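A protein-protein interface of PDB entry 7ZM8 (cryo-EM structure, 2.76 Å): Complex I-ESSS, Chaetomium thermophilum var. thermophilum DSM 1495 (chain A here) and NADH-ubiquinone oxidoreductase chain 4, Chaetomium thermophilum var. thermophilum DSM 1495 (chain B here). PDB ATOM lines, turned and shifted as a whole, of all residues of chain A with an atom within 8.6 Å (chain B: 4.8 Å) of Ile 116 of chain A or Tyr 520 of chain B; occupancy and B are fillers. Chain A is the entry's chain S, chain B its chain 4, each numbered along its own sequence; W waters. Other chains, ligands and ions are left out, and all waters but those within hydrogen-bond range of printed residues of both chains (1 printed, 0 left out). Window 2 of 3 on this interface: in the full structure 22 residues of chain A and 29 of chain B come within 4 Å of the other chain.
Water W1 lies within hydrogen-bond range of the backbone carbonyl oxygen of Phe 99 of chain B (2.9 Å) and the backbone NH of Ile 116 of chain A (3.2 Å).
CG2 of Ile 116 of chain A touches CB of His 519 of chain B (3.8 Å). Ile 116 of chain A touches Tyr 520 of chain B. NE2 of Gln 117 of chain A touches CD2 of His 519 of chain B, at 3.0 Å.
The backbone NH (N) of Phe 99 of chain B is in hydrogen-bond range of the side-chain hydroxyl (OG1) of Thr 114 of chain A. O of Thr 114 of chain A is in hydrogen-bond range of OG of Ser 100 of chain B (2.7 Å).
Hydrophobic or aromatic side chains of chain B within 4 Å of the printed part of chain A: Phe 99, His 519 and Tyr 520. Of the 11 printed residues of chain A, 3 touch a printed residue of chain B. Hydrophobic or aromatic side chains of chain A within 4 Å of the printed part of chain B: Ile 116. Along chain A the printed residues that touch a printed residue of chain B span positions 114 to 117. Among the printed residues, 5 pairs touch across the chains.
Of the printed residues of chain B, Ile 116 of chain A touches His 519 and Tyr 520. Tyr 520 of chain B touches just one residue of chain A: Ile 116. Of the printed residues of chain B, Gln 117 of chain A touches His 519. Of the printed residues of chain A, His 519 of chain B touches Ile 116 and Gln 117. Of the printed residues of chain A, Ser 100 of chain B touches Thr 114 (2.7 Å). Of the printed residues of chain B, Thr 114 of chain A touches Phe 99 and Ser 100. The nearest residue of chain A that does not touch Tyr 520 of chain B is Gln 117 of chain A (5.9 Å). The nearest printed residue of chain B that does not touch Gln 117 of chain A is Tyr 520 of chain B (5.9 Å).
The side-chain amide nitrogen (NE2) of Gln 117 of chain A is in hydrogen-bond range of the side-chain hydroxyl (OG) of Ser 115 of chain A, 2.7 Å away. The backbone carbonyl oxygen (O) of His 519 of chain B is in hydrogen-bond range of the side-chain hydroxyl (OG) of Ser 523 of chain B, at 2.8 Å.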
ATOM      1  N   ASP A 113      14.255  -5.796  15.163  1.00  0.00           N
ATOM      2  CA  ASP A 113      15.596  -6.367  15.236  1.00  0.00           C
ATOM      3  C   ASP A 113      15.756  -7.114  16.550  1.00  0.00           C
ATOM      4  O   ASP A 113      15.939  -6.504  17.606  1.00  0.00           O
ATOM      5  CB  ASP A 113      16.662  -5.289  15.092  1.00  0.00           C
ATOM      6  CG  ASP A 113      18.054  -5.868  15.010  1.00  0.00           C
ATOM      7  OD1 ASP A 113      18.233  -6.887  14.314  1.00  0.00           O
ATOM      8  OD2 ASP A 113      18.969  -5.318  15.646  1.00  0.00           O
ATOM      9  N   THR A 114      15.705  -8.441  16.481  1.00  0.00           N
ATOM     10  CA  THR A 114      15.875  -9.302  17.640  1.00  0.00           C
ATOM     11  C   THR A 114      17.223 -10.010  17.637  1.00  0.00           C
ATOM     12  O   THR A 114      17.369 -11.062  18.259  1.00  0.00           O
ATOM     13  CB  THR A 114      14.729 -10.311  17.719  1.00  0.00           C
ATOM     14  OG1 THR A 114      14.914 -11.334  16.737  1.00  0.00           O
ATOM     15  CG2 THR A 114      13.395  -9.627  17.480  1.00  0.00           C
ATOM     16  N   SER A 115      18.229  -9.422  17.000  1.00  0.00           N
ATOM     17  CA  SER A 115      19.611  -9.972  16.998  1.00  0.00           C
ATOM     18  C   SER A 115      20.254  -9.845  18.388  1.00  0.00           C
ATOM     19  O   SER A 115      19.901  -8.917  19.110  1.00  0.00           O
ATOM     20  CB  SER A 115      20.426  -9.261  15.962  1.00  0.00           C
ATOM     21  OG  SER A 115      21.635  -9.949  15.706  1.00  0.00           O
ATOM     22  N   ILE A 116      21.164 -10.747  18.746  1.00  0.00           N
ATOM     23  CA  ILE A 116      21.873 -10.714  20.063  1.00  0.00           C
ATOM     24  C   ILE A 116      22.751  -9.473  20.168  1.00  0.00           C
ATOM     25  O   ILE A 116      22.921  -8.975  21.276  1.00  0.00           O
ATOM     26  CB  ILE A 116      22.692 -12.000  20.337  1.00  0.00           C
ATOM     27  CG1 ILE A 116      23.161 -12.094  21.791  1.00  0.00           C
ATOM     28  CG2 ILE A 116      23.835 -12.189  19.356  1.00  0.00           C
ATOM     29  CD1 ILE A 116      22.039 -12.056  22.792  1.00  0.00           C
ATOM     30  N   GLN A 117      23.255  -8.973  19.051  1.00  0.00           N
ATOM     31  CA  GLN A 117      24.239  -7.878  19.124  1.00  0.00           C
ATOM     32  C   GLN A 117      23.523  -6.574  19.457  1.00  0.00           C
ATOM     33  O   GLN A 117      23.963  -5.919  20.393  1.00  0.00           O
ATOM     34  CB  GLN A 117      25.025  -7.818  17.816  1.00  0.00           C
ATOM     35  CG  GLN A 117      25.575  -9.164  17.378  1.00  0.00           C
ATOM     36  CD  GLN A 117      24.798  -9.719  16.214  1.00  0.00           C
ATOM     37  OE1 GLN A 117      24.836  -9.191  15.108  1.00  0.00           O
ATOM     38  NE2 GLN A 117      24.077 -10.797  16.457  1.00  0.00           N
ATOM     39  N   THR A 118      22.417  -6.257  18.799  1.00  0.00           N
ATOM     40  CA  THR A 118      21.750  -5.020  19.183  1.00  0.00           C
ATOM     41  C   THR A 118      21.426  -4.999  20.666  1.00  0.00           C
ATOM     42  O   THR A 118      21.413  -3.930  21.283  1.00  0.00           O
ATOM     43  CB  THR A 118      20.484  -4.817  18.348  1.00  0.00           C
ATOM     44  OG1 THR A 118      20.044  -3.458  18.461  1.00  0.00           O
ATOM     45  CG2 THR A 118      19.366  -5.746  18.795  1.00  0.00           C
ATOM     46  N   TRP A 119      21.177  -6.169  21.256  1.00  0.00           N
ATOM     47  CA  TRP A 119      20.943  -6.261  22.687  1.00  0.00           C
ATOM     48  C   TRP A 119      22.244  -6.162  23.466  1.00  0.00           C
ATOM     49  O   TRP A 119      22.296  -5.520  24.518  1.00  0.00           O
ATOM     50  CB  TRP A 119      20.219  -7.565  23.005  1.00  0.00           C
ATOM     51  CG  TRP A 119      19.802  -7.679  24.435  1.00  0.00           C
ATOM     52  CD1 TRP A 119      18.583  -7.392  24.946  1.00  0.00           C
ATOM     53  CD2 TRP A 119      20.599  -8.143  25.529  1.00  0.00           C
ATOM     54  NE1 TRP A 119      18.568  -7.627  26.290  1.00  0.00           N
ATOM     55  CE2 TRP A 119      19.795  -8.092  26.675  1.00  0.00           C
ATOM     56  CE3 TRP A 119      21.913  -8.600  25.649  1.00  0.00           C
ATOM     57  CZ2 TRP A 119      20.260  -8.470  27.927  1.00  0.00           C
ATOM     58  CZ3 TRP A 119      22.377  -8.960  26.886  1.00  0.00           C
ATOM     59  CH2 TRP A 119      21.554  -8.898  28.011  1.00  0.00           C
ATOM     60  N   ALA A 120      23.297  -6.795  22.965  1.00  0.00           N
ATOM     61  CA  ALA A 120      24.561  -6.817  23.679  1.00  0.00           C
ATOM     62  C   ALA A 120      25.318  -5.502  23.556  1.00  0.00           C
ATOM     63  O   ALA A 120      26.059  -5.147  24.473  1.00  0.00           O
ATOM     64  CB  ALA A 120      25.419  -7.980  23.184  1.00  0.00           C
ATOM     65  N   LEU A 121      25.165  -4.776  22.443  1.00  0.00           N
ATOM     66  CA  LEU A 121      25.811  -3.471  22.339  1.00  0.00           C
ATOM     67  C   LEU A 121      25.279  -2.503  23.383  1.00  0.00           C
ATOM     68  O   LEU A 121      26.051  -1.759  23.997  1.00  0.00           O
ATOM     69  CB  LEU A 121      25.631  -2.855  20.952  1.00  0.00           C
ATOM     70  CG  LEU A 121      26.499  -3.171  19.730  1.00  0.00           C
ATOM     71  CD1 LEU A 121      27.943  -2.750  19.957  1.00  0.00           C
ATOM     72  CD2 LEU A 121      26.401  -4.584  19.239  1.00  0.00           C
ATOM     73  N   GLU A 122      23.964  -2.483  23.587  1.00  0.00           N
ATOM     74  CA  GLU A 122      23.375  -1.478  24.463  1.00  0.00           C
ATOM     75  C   GLU A 122      23.767  -1.707  25.917  1.00  0.00           C
ATOM     76  O   GLU A 122      24.000  -0.748  26.659  1.00  0.00           O
ATOM     77  CB  GLU A 122      21.860  -1.477  24.303  1.00  0.00           C
ATOM     78  CG  GLU A 122      21.148  -0.488  25.194  1.00  0.00           C
ATOM     79  CD  GLU A 122      19.694  -0.824  25.365  1.00  0.00           C
ATOM     80  OE1 GLU A 122      19.164  -0.630  26.478  1.00  0.00           O
ATOM     81  OE2 GLU A 122      19.090  -1.301  24.385  1.00  0.00           O
ATOM     82  N   GLU A 123      23.832  -2.970  26.345  1.00  0.00           N
ATOM     83  CA  GLU A 123      24.348  -3.276  27.673  1.00  0.00           C
ATOM     84  C   GLU A 123      25.831  -2.976  27.766  1.00  0.00           C
ATOM     85  O   GLU A 123      26.282  -2.337  28.723  1.00  0.00           O
ATOM     86  CB  GLU A 123      24.087  -4.739  28.022  1.00  0.00           C
ATOM     87  CG  GLU A 123      24.460  -5.110  29.446  1.00  0.00           C
ATOM     88  CD  GLU A 123      24.012  -4.069  30.464  1.00  0.00           C
ATOM     89  OE1 GLU A 123      22.809  -3.742  30.511  1.00  0.00           O
ATOM     90  OE2 GLU A 123      24.871  -3.567  31.218  1.00  0.00           O
ATOM     91  N   PHE B  99      15.233 -13.868  16.410  1.00  0.00           N
ATOM     92  CA  PHE B  99      16.654 -14.197  16.136  1.00  0.00           C
ATOM     93  C   PHE B  99      17.452 -14.417  17.415  1.00  0.00           C
ATOM     94  O   PHE B  99      18.572 -14.897  17.287  1.00  0.00           O
ATOM     95  CB  PHE B  99      17.346 -13.087  15.348  1.00  0.00           C
ATOM     96  CG  PHE B  99      16.953 -12.920  13.906  1.00  0.00           C
ATOM     97  CD1 PHE B  99      16.349 -13.946  13.202  1.00  0.00           C
ATOM     98  CD2 PHE B  99      17.231 -11.737  13.246  1.00  0.00           C
ATOM     99  CE1 PHE B  99      16.010 -13.780  11.871  1.00  0.00           C
ATOM    100  CE2 PHE B  99      16.889 -11.572  11.914  1.00  0.00           C
ATOM    101  CZ  PHE B  99      16.279 -12.595  11.233  1.00  0.00           C
ATOM    102  N   SER B 100      16.951 -14.048  18.591  1.00  0.00           N
ATOM    103  CA  SER B 100      17.725 -14.368  19.817  1.00  0.00           C
ATOM    104  C   SER B 100      16.851 -15.051  20.865  1.00  0.00           C
ATOM    105  O   SER B 100      16.729 -14.502  21.955  1.00  0.00           O
ATOM    106  CB  SER B 100      18.394 -13.156  20.367  1.00  0.00           C
ATOM    107  OG  SER B 100      17.450 -12.149  20.695  1.00  0.00           O
ATOM    108  N   ASN B 101      16.346 -16.247  20.569  1.00  0.00           N
ATOM    109  CA  ASN B 101      15.458 -16.993  21.496  1.00  0.00           C
ATOM    110  C   ASN B 101      15.996 -18.411  21.678  1.00  0.00           C
ATOM    111  O   ASN B 101      16.338 -19.026  20.677  1.00  0.00           O
ATOM    112  CB  ASN B 101      14.014 -16.982  20.998  1.00  0.00           C
ATOM    113  CG  ASN B 101      12.985 -17.346  22.046  1.00  0.00           C
ATOM    114  OD1 ASN B 101      13.311 -17.544  23.212  1.00  0.00           O
ATOM    115  ND2 ASN B 101      11.731 -17.423  21.640  1.00  0.00           N
ATOM    116  N   ASN B 102      16.073 -18.902  22.909  1.00  0.00           N
ATOM    117  CA  ASN B 102      16.646 -20.245  23.173  1.00  0.00           C
ATOM    118  C   ASN B 102      15.540 -21.291  23.269  1.00  0.00           C
ATOM    119  O   ASN B 102      15.864 -22.457  23.495  1.00  0.00           O
ATOM    120  CB  ASN B 102      17.621 -20.265  24.352  1.00  0.00           C
ATOM    121  CG  ASN B 102      16.985 -20.313  25.721  1.00  0.00           C
ATOM    122  OD1 ASN B 102      15.851 -19.884  25.921  1.00  0.00           O
ATOM    123  ND2 ASN B 102      17.735 -20.822  26.680  1.00  0.00           N
ATOM    124  N   LEU B 518      21.719 -16.833  13.097  1.00  0.00           N
ATOM    125  CA  LEU B 518      22.469 -17.974  13.685  1.00  0.00           C
ATOM    126  C   LEU B 518      23.267 -17.644  14.949  1.00  0.00           C
ATOM    127  O   LEU B 518      23.503 -18.572  15.705  1.00  0.00           O
ATOM    128  CB  LEU B 518      23.483 -18.456  12.641  1.00  0.00           C
ATOM    129  CG  LEU B 518      22.961 -18.893  11.280  1.00  0.00           C
ATOM    130  CD1 LEU B 518      24.112 -18.949  10.293  1.00  0.00           C
ATOM    131  CD2 LEU B 518      22.292 -20.249  11.375  1.00  0.00           C
ATOM    132  N   HIS B 519      23.666 -16.396  15.174  1.00  0.00           N
ATOM    133  CA  HIS B 519      24.581 -16.036  16.300  1.00  0.00           C
ATOM    134  C   HIS B 519      24.216 -16.669  17.647  1.00  0.00           C
ATOM    135  O   HIS B 519      25.054 -17.421  18.159  1.00  0.00           O
ATOM    136  CB  HIS B 519      24.688 -14.512  16.422  1.00  0.00           C
ATOM    137  CG  HIS B 519      25.554 -13.869  15.396  1.00  0.00           C
ATOM    138  ND1 HIS B 519      26.818 -14.331  15.109  1.00  0.00           N
ATOM    139  CD2 HIS B 519      25.357 -12.794  14.607  1.00  0.00           C
ATOM    140  CE1 HIS B 519      27.352 -13.579  14.171  1.00  0.00           C
ATOM    141  NE2 HIS B 519      26.478 -12.627  13.849  1.00  0.00           N
ATOM    142  N   TYR B 520      23.045 -16.358  18.205  1.00  0.00           N
ATOM    143  CA  TYR B 520      22.617 -16.815  19.549  1.00  0.00           C
ATOM    144  C   TYR B 520      22.476 -18.339  19.591  1.00  0.00           C
ATOM    145  O   TYR B 520      22.857 -18.955  20.589  1.00  0.00           O
ATOM    146  CB  TYR B 520      21.323 -16.077  19.880  1.00  0.00           C
ATOM    147  CG  TYR B 520      20.740 -16.383  21.230  1.00  0.00           C
ATOM    148  CD1 TYR B 520      21.150 -15.688  22.351  1.00  0.00           C
ATOM    149  CD2 TYR B 520      19.781 -17.363  21.377  1.00  0.00           C
ATOM    150  CE1 TYR B 520      20.628 -15.965  23.599  1.00  0.00           C
ATOM    151  CE2 TYR B 520      19.251 -17.656  22.617  1.00  0.00           C
ATOM    152  CZ  TYR B 520      19.675 -16.956  23.727  1.00  0.00           C
ATOM    153  OH  TYR B 520      19.145 -17.250  24.942  1.00  0.00           O
ATOM    154  N   ASN B 521      21.874 -18.922  18.567  1.00  0.00           N
ATOM    155  CA  ASN B 521      21.654 -20.389  18.488  1.00  0.00           C
ATOM    156  C   ASN B 521      22.973 -21.140  18.267  1.00  0.00           C
ATOM    157  O   ASN B 521      23.077 -22.269  18.737  1.00  0.00           O
ATOM    158  CB  ASN B 521      20.483 -20.725  17.559  1.00  0.00           C
ATOM    159  CG  ASN B 521      19.173 -20.115  18.019  1.00  0.00           C
ATOM    160  OD1 ASN B 521      18.414 -19.588  17.218  1.00  0.00           O
ATOM    161  ND2 ASN B 521      18.897 -20.158  19.310  1.00  0.00           N
ATOM    162  N   ILE B 522      23.902 -20.584  17.498  1.00  0.00           N
ATOM    163  CA  ILE B 522      25.242 -21.200  17.319  1.00  0.00           C
ATOM    164  C   ILE B 522      25.934 -21.148  18.678  1.00  0.00           C
ATOM    165  O   ILE B 522      26.686 -22.073  19.000  1.00  0.00           O
ATOM    166  CB  ILE B 522      26.043 -20.508  16.188  1.00  0.00           C
ATOM    167  CG1 ILE B 522      25.455 -20.801  14.806  1.00  0.00           C
ATOM    168  CG2 ILE B 522      27.518 -20.872  16.237  1.00  0.00           C
ATOM    169  CD1 ILE B 522      25.873 -22.123  14.234  1.00  0.00           C
ATOM    170  N   SER B 523      25.656 -20.115  19.459  1.00  0.00           N
ATOM    171  CA  SER B 523      26.364 -19.931  20.745  1.00  0.00           C
ATOM    172  C   SER B 523      26.102 -21.127  21.646  1.00  0.00           C
ATOM    173  O   SER B 523      26.916 -21.357  22.537  1.00  0.00           O
ATOM    174  CB  SER B 523      25.969 -18.636  21.390  1.00  0.00           C
ATOM    175  OG  SER B 523      26.371 -17.553  20.576  1.00  0.00           O
ATOM    176  N   SER B 524      25.005 -21.836  21.433  1.00  0.00           N
ATOM    177  CA  SER B 524      24.611 -22.973  22.295  1.00  0.00           C
ATOM    178  C   SER B 524      25.367 -24.273  21.994  1.00  0.00           C
ATOM    179  O   SER B 524      25.234 -25.193  22.797  1.00  0.00           O
ATOM    180  CB  SER B 524      23.129 -23.162  22.229  1.00  0.00           C
ATOM    181  OG  SER B 524      22.723 -23.636  20.956  1.00  0.00           O
HETATM  182  O   HOH W   1      21.137 -13.504  17.135  1.00  0.00           O
